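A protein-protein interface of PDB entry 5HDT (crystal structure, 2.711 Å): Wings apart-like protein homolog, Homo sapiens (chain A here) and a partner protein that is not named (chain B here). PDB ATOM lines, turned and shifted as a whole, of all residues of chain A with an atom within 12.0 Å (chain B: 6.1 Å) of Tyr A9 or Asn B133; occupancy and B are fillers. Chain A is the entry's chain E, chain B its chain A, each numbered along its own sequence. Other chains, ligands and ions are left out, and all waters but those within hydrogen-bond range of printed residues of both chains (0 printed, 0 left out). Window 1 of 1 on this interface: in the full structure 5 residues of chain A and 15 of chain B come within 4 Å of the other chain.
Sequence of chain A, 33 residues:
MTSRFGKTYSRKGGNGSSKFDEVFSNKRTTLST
OH of Tyr A9 sits at hydrogen-bond distance from O of Phe B79 (2.6 Å).
The backbone carbonyl oxygen of Val B129 lies close to the backbone NH of Tyr A9, 3.4 Å away.
The side-chain amide nitrogen (ND2) of Asn B133 sits at hydrogen-bond distance from the backbone carbonyl oxygen (O) of Tyr A9 (3.2 Å).
The guanidinium group (NH1) of Arg A11 lies within salt-bridge range of the side-chain carboxylate (OE1) of Glu B137, 3.2 Å away.
The guanidinium group (NE) of Arg A11 is in hydrogen-bond range of the backbone carbonyl oxygen (O) of Glu B178.
OG of Ser B174 lies within hydrogen-bond range of ND2 of Asn B133 (2.8 Å).
ND2 of Asn B133 lies within hydrogen-bond range of OE1 of Glu B178, 2.8 Å away.
The side-chain carboxylate (OE1) of Glu B178 sits at hydrogen-bond distance from the side-chain hydroxyl (OG) of Ser B174, at 3.2 Å.
Among the printed residues, merely in contact across the chains: Thr A8 with Val B129 (3.3 Å), Tyr A9 with Ala B83 (3.5 Å), Tyr A9 with Pro B84 (3.8 Å), Tyr A9 with Lys B130 (3.4 Å), Tyr A9 with Ser B131 (3.95 Å), Tyr A9 with Ile B134 (3.6 Å), Tyr A9 with Glu B178 (3.6 Å), Ser A10 with Glu B178 (3.3 Å) and Arg A11 with Phe B136 (3.7 Å).
Of chain B, only Phe B79, Ala B83, Pro B84, Val B129, Lys B130, Ser B131, Asn B133, Ile B134 and Glu B178 come within 4 Å of Tyr A9.
Of the printed residues of chain A, Asn B133 touches Tyr A9.
Phe B79 touches just one residue of chain A: Tyr A9 (2.6 Å).
Pro B84 touches one residue of chain A.
No residue of chain A comes within 4 Å of Ala B86.
Val B129 touches just these residues of chain A: Thr A8 (3.3 Å) and Tyr A9 (3.3 Å).
Ile B134 touches just one residue of chain A: Tyr A9 (3.6 Å).
No residue of chain A comes within 4 Å of Cys B135.
Phe B136 touches just one residue of chain A: Arg A11.
No residue of chain A comes within 4 Å of Ser B174.
Ile B175 touches none of the printed residues of chain A.
Of the printed residues of chain A, Glu B137 touches Arg A11 (3.2 Å).
Of the printed residues of chain B, Thr A8 touches Val B129 (3.3 Å).
Of the printed residues of chain B, Ser A10 touches Glu B178.
Of the printed residues of chain B, Arg A11 touches Phe B136 (3.7 Å), Glu B137 (3.2 Å) and Glu B178 (3.1 Å).
Lys A7 touches none of the printed residues of chain B.
The nearest residue of chain B that does not touch Tyr A9 is Ala B86 (4.3 Å).
Of the 5 printed residues of chain A, 4 touch a printed residue of chain B.
Hydrophobic or aromatic side chains of chain A within 4 Å of the printed part of chain B: Tyr A9.
Of the 23 printed residues of chain B, 11 touch a printed residue of chain A.
Among the printed residues, Asp or Glu carboxylates within 4 Å of a Lys or Arg side-chain nitrogen of the other chain: Arg A11 with Glu B137.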
ATOM      1  N   LYS A   7      -7.819 -24.068   8.650  1.00  0.00           N
ATOM      2  CA  LYS A   7      -7.044 -24.086   9.885  1.00  0.00           C
ATOM      3  C   LYS A   7      -6.427 -22.717  10.156  1.00  0.00           C
ATOM      4  O   LYS A   7      -5.842 -22.101   9.263  1.00  0.00           O
ATOM      5  CB  LYS A   7      -5.951 -25.155   9.818  1.00  0.00           C
ATOM      6  CG  LYS A   7      -6.485 -26.578   9.769  1.00  0.00           C
ATOM      7  CD  LYS A   7      -5.357 -27.589   9.655  1.00  0.00           C
ATOM      8  CE  LYS A   7      -5.883 -29.015   9.647  1.00  0.00           C
ATOM      9  NZ  LYS A   7      -4.785 -30.009   9.485  1.00  0.00           N
ATOM     10  N   THR A   8      -6.571 -22.246  11.392  1.00  0.00           N
ATOM     11  CA  THR A   8      -6.071 -20.934  11.788  1.00  0.00           C
ATOM     12  C   THR A   8      -5.570 -20.955  13.230  1.00  0.00           C
ATOM     13  O   THR A   8      -5.701 -21.963  13.928  1.00  0.00           O
ATOM     14  CB  THR A   8      -7.163 -19.853  11.653  1.00  0.00           C
ATOM     15  OG1 THR A   8      -8.236 -20.133  12.561  1.00  0.00           O
ATOM     16  CG2 THR A   8      -7.707 -19.807  10.232  1.00  0.00           C
ATOM     17  N   TYR A   9      -5.000 -19.836  13.666  1.00  0.00           N
ATOM     18  CA  TYR A   9      -4.527 -19.691  15.039  1.00  0.00           C
ATOM     19  C   TYR A   9      -5.608 -19.051  15.906  1.00  0.00           C
ATOM     20  O   TYR A   9      -5.957 -17.887  15.709  1.00  0.00           O
ATOM     21  CB  TYR A   9      -3.253 -18.846  15.085  1.00  0.00           C
ATOM     22  CG  TYR A   9      -2.208 -19.229  14.063  1.00  0.00           C
ATOM     23  CD1 TYR A   9      -2.273 -18.750  12.762  1.00  0.00           C
ATOM     24  CD2 TYR A   9      -1.148 -20.061  14.402  1.00  0.00           C
ATOM     25  CE1 TYR A   9      -1.319 -19.092  11.826  1.00  0.00           C
ATOM     26  CE2 TYR A   9      -0.188 -20.409  13.472  1.00  0.00           C
ATOM     27  CZ  TYR A   9      -0.279 -19.923  12.185  1.00  0.00           C
ATOM     28  OH  TYR A   9       0.674 -20.265  11.254  1.00  0.00           O
ATOM     29  N   SER A  10      -6.134 -19.812  16.863  1.00  0.00           N
ATOM     30  CA  SER A  10      -7.186 -19.313  17.746  1.00  0.00           C
ATOM     31  C   SER A  10      -7.016 -19.814  19.177  1.00  0.00           C
ATOM     32  O   SER A  10      -6.366 -20.834  19.418  1.00  0.00           O
ATOM     33  CB  SER A  10      -8.563 -19.720  17.219  1.00  0.00           C
ATOM     34  OG  SER A  10      -8.827 -19.120  15.965  1.00  0.00           O
ATOM     35  N   ARG A  11      -7.610 -19.086  20.119  1.00  0.00           N
ATOM     36  CA  ARG A  11      -7.519 -19.422  21.536  1.00  0.00           C
ATOM     37  C   ARG A  11      -8.860 -19.216  22.234  1.00  0.00           C
ATOM     38  O   ARG A  11      -9.351 -18.092  22.344  1.00  0.00           O
ATOM     39  CB  ARG A  11      -6.439 -18.577  22.215  1.00  0.00           C
ATOM     40  CG  ARG A  11      -5.137 -18.483  21.429  1.00  0.00           C
ATOM     41  CD  ARG A  11      -3.962 -18.195  22.342  1.00  0.00           C
ATOM     42  NE  ARG A  11      -4.231 -17.088  23.254  1.00  0.00           N
ATOM     43  CZ  ARG A  11      -3.393 -16.677  24.201  1.00  0.00           C
ATOM     44  NH1 ARG A  11      -2.224 -17.278  24.373  1.00  0.00           N
ATOM     45  NH2 ARG A  11      -3.723 -15.661  24.984  1.00  0.00           N
ATOM     46  N   ILE B  78       2.992 -18.981   4.022  1.00  0.00           N
ATOM     47  CA  ILE B  78       3.845 -19.892   4.778  1.00  0.00           C
ATOM     48  C   ILE B  78       3.297 -20.096   6.189  1.00  0.00           C
ATOM     49  O   ILE B  78       3.456 -21.168   6.771  1.00  0.00           O
ATOM     50  CB  ILE B  78       5.293 -19.373   4.844  1.00  0.00           C
ATOM     51  CG1 ILE B  78       5.957 -19.518   3.476  1.00  0.00           C
ATOM     52  CG2 ILE B  78       6.113 -20.149   5.878  1.00  0.00           C
ATOM     53  CD1 ILE B  78       7.265 -18.768   3.338  1.00  0.00           C
ATOM     54  N   PHE B  79       2.655 -19.067   6.736  1.00  0.00           N
ATOM     55  CA  PHE B  79       1.985 -19.185   8.029  1.00  0.00           C
ATOM     56  C   PHE B  79       0.665 -19.936   7.873  1.00  0.00           C
ATOM     57  O   PHE B  79       0.258 -20.678   8.765  1.00  0.00           O
ATOM     58  CB  PHE B  79       1.738 -17.802   8.647  1.00  0.00           C
ATOM     59  CG  PHE B  79       2.948 -17.202   9.315  1.00  0.00           C
ATOM     60  CD1 PHE B  79       3.671 -17.923  10.253  1.00  0.00           C
ATOM     61  CD2 PHE B  79       3.359 -15.915   9.009  1.00  0.00           C
ATOM     62  CE1 PHE B  79       4.782 -17.373  10.867  1.00  0.00           C
ATOM     63  CE2 PHE B  79       4.469 -15.360   9.619  1.00  0.00           C
ATOM     64  CZ  PHE B  79       5.181 -16.090  10.549  1.00  0.00           C
ATOM     65  N   ARG B  80       0.005 -19.739   6.737  1.00  0.00           N
ATOM     66  CA  ARG B  80      -1.266 -20.401   6.460  1.00  0.00           C
ATOM     67  C   ARG B  80      -1.077 -21.905   6.327  1.00  0.00           C
ATOM     68  O   ARG B  80      -1.808 -22.691   6.929  1.00  0.00           O
ATOM     69  CB  ARG B  80      -1.892 -19.847   5.179  1.00  0.00           C
ATOM     70  CG  ARG B  80      -3.255 -20.442   4.837  1.00  0.00           C
ATOM     71  CD  ARG B  80      -3.757 -19.954   3.484  1.00  0.00           C
ATOM     72  NE  ARG B  80      -2.840 -20.305   2.401  1.00  0.00           N
ATOM     73  CZ  ARG B  80      -2.756 -21.513   1.848  1.00  0.00           C
ATOM     74  NH1 ARG B  80      -3.529 -22.503   2.273  1.00  0.00           N
ATOM     75  NH2 ARG B  80      -1.888 -21.735   0.869  1.00  0.00           N
ATOM     76  N   TYR B  82       1.376 -23.972   7.242  1.00  0.00           N
ATOM     77  CA  TYR B  82       1.994 -24.739   8.319  1.00  0.00           C
ATOM     78  C   TYR B  82       1.230 -24.636   9.641  1.00  0.00           C
ATOM     79  O   TYR B  82       1.632 -25.229  10.639  1.00  0.00           O
ATOM     80  CB  TYR B  82       3.441 -24.279   8.524  1.00  0.00           C
ATOM     81  CG  TYR B  82       4.390 -24.662   7.404  1.00  0.00           C
ATOM     82  CD1 TYR B  82       3.933 -24.867   6.107  1.00  0.00           C
ATOM     83  CD2 TYR B  82       5.743 -24.833   7.652  1.00  0.00           C
ATOM     84  CE1 TYR B  82       4.798 -25.219   5.092  1.00  0.00           C
ATOM     85  CE2 TYR B  82       6.617 -25.188   6.641  1.00  0.00           C
ATOM     86  CZ  TYR B  82       6.137 -25.379   5.364  1.00  0.00           C
ATOM     87  OH  TYR B  82       6.993 -25.732   4.348  1.00  0.00           O
ATOM     88  N   ALA B  83       0.129 -23.892   9.646  1.00  0.00           N
ATOM     89  CA  ALA B  83      -0.630 -23.667  10.875  1.00  0.00           C
ATOM     90  C   ALA B  83      -1.220 -24.968  11.413  1.00  0.00           C
ATOM     91  O   ALA B  83      -1.490 -25.886  10.641  1.00  0.00           O
ATOM     92  CB  ALA B  83      -1.738 -22.658  10.630  1.00  0.00           C
ATOM     93  N   PRO B  84      -1.431 -25.050  12.742  1.00  0.00           N
ATOM     94  CA  PRO B  84      -1.084 -24.046  13.758  1.00  0.00           C
ATOM     95  C   PRO B  84       0.363 -24.138  14.257  1.00  0.00           C
ATOM     96  O   PRO B  84       0.663 -23.603  15.325  1.00  0.00           O
ATOM     97  CB  PRO B  84      -2.061 -24.355  14.907  1.00  0.00           C
ATOM     98  CG  PRO B  84      -3.071 -25.305  14.342  1.00  0.00           C
ATOM     99  CD  PRO B  84      -2.344 -26.064  13.290  1.00  0.00           C
ATOM    100  N   GLU B  85       1.236 -24.801  13.501  1.00  0.00           N
ATOM    101  CA  GLU B  85       2.635 -24.957  13.895  1.00  0.00           C
ATOM    102  C   GLU B  85       3.580 -24.350  12.858  1.00  0.00           C
ATOM    103  O   GLU B  85       4.048 -25.034  11.947  1.00  0.00           O
ATOM    104  CB  GLU B  85       2.967 -26.437  14.104  1.00  0.00           C
ATOM    105  CG  GLU B  85       4.375 -26.697  14.625  1.00  0.00           C
ATOM    106  CD  GLU B  85       4.622 -26.080  15.992  1.00  0.00           C
ATOM    107  OE1 GLU B  85       3.639 -25.780  16.701  1.00  0.00           O
ATOM    108  OE2 GLU B  85       5.803 -25.896  16.356  1.00  0.00           O
ATOM    109  N   ALA B  86       3.862 -23.060  13.016  1.00  0.00           N
ATOM    110  CA  ALA B  86       4.724 -22.337  12.088  1.00  0.00           C
ATOM    111  C   ALA B  86       6.130 -22.941  12.046  1.00  0.00           C
ATOM    112  O   ALA B  86       6.537 -23.635  12.979  1.00  0.00           O
ATOM    113  CB  ALA B  86       4.789 -20.868  12.478  1.00  0.00           C
ATOM    114  N   PHE B  98       6.825 -10.096  11.627  1.00  0.00           N
ATOM    115  CA  PHE B  98       5.526  -9.456  11.780  1.00  0.00           C
ATOM    116  C   PHE B  98       5.631  -7.937  11.781  1.00  0.00           C
ATOM    117  O   PHE B  98       4.700  -7.251  11.364  1.00  0.00           O
ATOM    118  CB  PHE B  98       4.840  -9.959  13.048  1.00  0.00           C
ATOM    119  CG  PHE B  98       4.242 -11.324  12.891  1.00  0.00           C
ATOM    120  CD1 PHE B  98       3.139 -11.518  12.075  1.00  0.00           C
ATOM    121  CD2 PHE B  98       4.790 -12.417  13.534  1.00  0.00           C
ATOM    122  CE1 PHE B  98       2.589 -12.772  11.912  1.00  0.00           C
ATOM    123  CE2 PHE B  98       4.241 -13.674  13.379  1.00  0.00           C
ATOM    124  CZ  PHE B  98       3.139 -13.851  12.566  1.00  0.00           C
ATOM    125  N   VAL B 129      -6.229 -15.930   8.219  1.00  0.00           N
ATOM    126  CA  VAL B 129      -5.418 -16.918   8.923  1.00  0.00           C
ATOM    127  C   VAL B 129      -5.208 -16.567  10.397  1.00  0.00           C
ATOM    128  O   VAL B 129      -4.924 -17.444  11.212  1.00  0.00           O
ATOM    129  CB  VAL B 129      -4.044 -17.069   8.240  1.00  0.00           C
ATOM    130  CG1 VAL B 129      -3.175 -18.099   8.961  1.00  0.00           C
ATOM    131  CG2 VAL B 129      -4.226 -17.467   6.783  1.00  0.00           C
ATOM    132  N   LYS B 130      -5.357 -15.289  10.733  1.00  0.00           N
ATOM    133  CA  LYS B 130      -5.076 -14.803  12.082  1.00  0.00           C
ATOM    134  C   LYS B 130      -3.621 -15.089  12.445  1.00  0.00           C
ATOM    135  O   LYS B 130      -3.324 -15.559  13.542  1.00  0.00           O
ATOM    136  CB  LYS B 130      -6.013 -15.446  13.109  1.00  0.00           C
ATOM    137  CG  LYS B 130      -7.480 -15.450  12.709  1.00  0.00           C
ATOM    138  CD  LYS B 130      -8.020 -14.039  12.524  1.00  0.00           C
ATOM    139  CE  LYS B 130      -9.476 -14.053  12.073  1.00  0.00           C
ATOM    140  NZ  LYS B 130     -10.356 -14.769  13.042  1.00  0.00           N
ATOM    141  N   SER B 131      -2.723 -14.793  11.509  1.00  0.00           N
ATOM    142  CA  SER B 131      -1.302 -15.078  11.675  1.00  0.00           C
ATOM    143  C   SER B 131      -0.701 -14.316  12.854  1.00  0.00           C
ATOM    144  O   SER B 131       0.177 -14.828  13.550  1.00  0.00           O
ATOM    145  CB  SER B 131      -0.544 -14.725  10.395  1.00  0.00           C
ATOM    146  OG  SER B 131      -1.143 -15.328   9.260  1.00  0.00           O
ATOM    147  N   TYR B 132      -1.178 -13.094  13.075  1.00  0.00           N
ATOM    148  CA  TYR B 132      -0.622 -12.231  14.112  1.00  0.00           C
ATOM    149  C   TYR B 132      -0.826 -12.781  15.519  1.00  0.00           C
ATOM    150  O   TYR B 132      -0.120 -12.385  16.446  1.00  0.00           O
ATOM    151  CB  TYR B 132      -1.233 -10.833  14.024  1.00  0.00           C
ATOM    152  CG  TYR B 132      -0.464  -9.881  13.146  1.00  0.00           C
ATOM    153  CD1 TYR B 132      -0.719  -9.803  11.790  1.00  0.00           C
ATOM    154  CD2 TYR B 132       0.516  -9.052  13.677  1.00  0.00           C
ATOM    155  CE1 TYR B 132      -0.023  -8.930  10.983  1.00  0.00           C
ATOM    156  CE2 TYR B 132       1.220  -8.174  12.875  1.00  0.00           C
ATOM    157  CZ  TYR B 132       0.947  -8.114  11.530  1.00  0.00           C
ATOM    158  OH  TYR B 132       1.650  -7.234  10.732  1.00  0.00           O
ATOM    159  N   ASN B 133      -1.786 -13.687  15.685  1.00  0.00           N
ATOM    160  CA  ASN B 133      -2.028 -14.295  16.991  1.00  0.00           C
ATOM    161  C   ASN B 133      -0.806 -15.052  17.494  1.00  0.00           C
ATOM    162  O   ASN B 133      -0.685 -15.336  18.686  1.00  0.00           O
ATOM    163  CB  ASN B 133      -3.229 -15.237  16.932  1.00  0.00           C
ATOM    164  CG  ASN B 133      -4.533 -14.503  16.700  1.00  0.00           C
ATOM    165  OD1 ASN B 133      -4.557 -13.431  16.095  1.00  0.00           O
ATOM    166  ND2 ASN B 133      -5.626 -15.076  17.188  1.00  0.00           N
ATOM    167  N   ILE B 134       0.097 -15.378  16.577  1.00  0.00           N
ATOM    168  CA  ILE B 134       1.356 -16.025  16.928  1.00  0.00           C
ATOM    169  C   ILE B 134       2.160 -15.162  17.899  1.00  0.00           C
ATOM    170  O   ILE B 134       2.951 -15.677  18.690  1.00  0.00           O
ATOM    171  CB  ILE B 134       2.202 -16.309  15.666  1.00  0.00           C
ATOM    172  CG1 ILE B 134       1.501 -17.346  14.788  1.00  0.00           C
ATOM    173  CG2 ILE B 134       3.598 -16.809  16.036  1.00  0.00           C
ATOM    174  CD1 ILE B 134       2.144 -17.536  13.428  1.00  0.00           C
ATOM    175  N   CYS B 135       1.943 -13.853  17.838  1.00  0.00           N
ATOM    176  CA  CYS B 135       2.732 -12.907  18.618  1.00  0.00           C
ATOM    177  C   CYS B 135       2.297 -12.793  20.082  1.00  0.00           C
ATOM    178  O   CYS B 135       2.950 -12.104  20.864  1.00  0.00           O
ATOM    179  CB  CYS B 135       2.674 -11.528  17.966  1.00  0.00           C
ATOM    180  SG  CYS B 135       3.312 -11.491  16.283  1.00  0.00           S
ATOM    181  N   PHE B 136       1.202 -13.453  20.456  1.00  0.00           N
ATOM    182  CA  PHE B 136       0.734 -13.412  21.841  1.00  0.00           C
ATOM    183  C   PHE B 136       1.818 -13.872  22.814  1.00  0.00           C
ATOM    184  O   PHE B 136       1.885 -13.398  23.948  1.00  0.00           O
ATOM    185  CB  PHE B 136      -0.512 -14.288  22.033  1.00  0.00           C
ATOM    186  CG  PHE B 136      -1.766 -13.736  21.407  1.00  0.00           C
ATOM    187  CD1 PHE B 136      -1.950 -12.374  21.235  1.00  0.00           C
ATOM    188  CD2 PHE B 136      -2.775 -14.594  21.004  1.00  0.00           C
ATOM    189  CE1 PHE B 136      -3.111 -11.884  20.661  1.00  0.00           C
ATOM    190  CE2 PHE B 136      -3.935 -14.111  20.429  1.00  0.00           C
ATOM    191  CZ  PHE B 136      -4.104 -12.758  20.258  1.00  0.00           C
ATOM    192  N   GLU B 137       2.666 -14.792  22.367  1.00  0.00           N
ATOM    193  CA  GLU B 137       3.669 -15.389  23.241  1.00  0.00           C
ATOM    194  C   GLU B 137       4.985 -14.608  23.244  1.00  0.00           C
ATOM    195  O   GLU B 137       5.841 -14.834  24.100  1.00  0.00           O
ATOM    196  CB  GLU B 137       3.923 -16.838  22.824  1.00  0.00           C
ATOM    197  CG  GLU B 137       2.662 -17.701  22.755  1.00  0.00           C
ATOM    198  CD  GLU B 137       1.985 -17.882  24.105  1.00  0.00           C
ATOM    199  OE1 GLU B 137       0.827 -18.354  24.130  1.00  0.00           O
ATOM    200  OE2 GLU B 137       2.606 -17.561  25.141  1.00  0.00           O
ATOM    201  N   PHE B 145       1.352  -5.197  18.214  1.00  0.00           N
ATOM    202  CA  PHE B 145      -0.075  -4.978  18.029  1.00  0.00           C
ATOM    203  C   PHE B 145      -0.407  -3.489  17.976  1.00  0.00           C
ATOM    204  O   PHE B 145      -1.295  -3.069  17.234  1.00  0.00           O
ATOM    205  CB  PHE B 145      -0.870  -5.650  19.151  1.00  0.00           C
ATOM    206  CG  PHE B 145      -0.766  -7.150  19.161  1.00  0.00           C
ATOM    207  CD1 PHE B 145      -0.552  -7.859  17.991  1.00  0.00           C
ATOM    208  CD2 PHE B 145      -0.889  -7.853  20.347  1.00  0.00           C
ATOM    209  CE1 PHE B 145      -0.462  -9.240  18.006  1.00  0.00           C
ATOM    210  CE2 PHE B 145      -0.799  -9.232  20.369  1.00  0.00           C
ATOM    211  CZ  PHE B 145      -0.584  -9.926  19.196  1.00  0.00           C
ATOM    212  N   LEU B 171      -8.997  -8.875  11.465  1.00  0.00           N
ATOM    213  CA  LEU B 171      -7.611  -8.949  11.902  1.00  0.00           C
ATOM    214  C   LEU B 171      -7.437  -8.405  13.320  1.00  0.00           C
ATOM    215  O   LEU B 171      -6.792  -9.034  14.156  1.00  0.00           O
ATOM    216  CB  LEU B 171      -6.722  -8.182  10.920  1.00  0.00           C
ATOM    217  CG  LEU B 171      -5.234  -8.059  11.234  1.00  0.00           C
ATOM    218  CD1 LEU B 171      -4.607  -9.424  11.470  1.00  0.00           C
ATOM    219  CD2 LEU B 171      -4.540  -7.340  10.091  1.00  0.00           C
ATOM    220  N   SER B 174      -9.546 -10.357  16.412  1.00  0.00           N
ATOM    221  CA  SER B 174      -8.937 -11.582  16.907  1.00  0.00           C
ATOM    222  C   SER B 174      -7.953 -11.293  18.034  1.00  0.00           C
ATOM    223  O   SER B 174      -7.948 -11.977  19.058  1.00  0.00           O
ATOM    224  CB  SER B 174      -8.236 -12.311  15.761  1.00  0.00           C
ATOM    225  OG  SER B 174      -7.733 -13.565  16.177  1.00  0.00           O
ATOM    226  N   ILE B 175      -7.135 -10.265  17.843  1.00  0.00           N
ATOM    227  CA  ILE B 175      -6.109  -9.899  18.813  1.00  0.00           C
ATOM    228  C   ILE B 175      -6.706  -9.540  20.177  1.00  0.00           C
ATOM    229  O   ILE B 175      -6.097  -9.804  21.214  1.00  0.00           O
ATOM    230  CB  ILE B 175      -5.266  -8.722  18.286  1.00  0.00           C
ATOM    231  CG1 ILE B 175      -4.455  -9.177  17.068  1.00  0.00           C
ATOM    232  CG2 ILE B 175      -4.328  -8.192  19.366  1.00  0.00           C
ATOM    233  CD1 ILE B 175      -3.760  -8.057  16.324  1.00  0.00           C
ATOM    234  N   GLU B 178      -9.118 -13.019  21.517  1.00  0.00           N
ATOM    235  CA  GLU B 178      -8.361 -14.228  21.822  1.00  0.00           C
ATOM    236  C   GLU B 178      -7.044 -13.920  22.534  1.00  0.00           C
ATOM    237  O   GLU B 178      -6.261 -14.823  22.822  1.00  0.00           O
ATOM    238  CB  GLU B 178      -8.108 -15.009  20.532  1.00  0.00           C
ATOM    239  CG  GLU B 178      -9.391 -15.553  19.908  1.00  0.00           C
ATOM    240  CD  GLU B 178      -9.240 -15.887  18.440  1.00  0.00           C
ATOM    241  OE1 GLU B 178      -8.097 -16.139  18.005  1.00  0.00           O
ATOM    242  OE2 GLU B 178     -10.261 -15.889  17.718  1.00  0.00           O
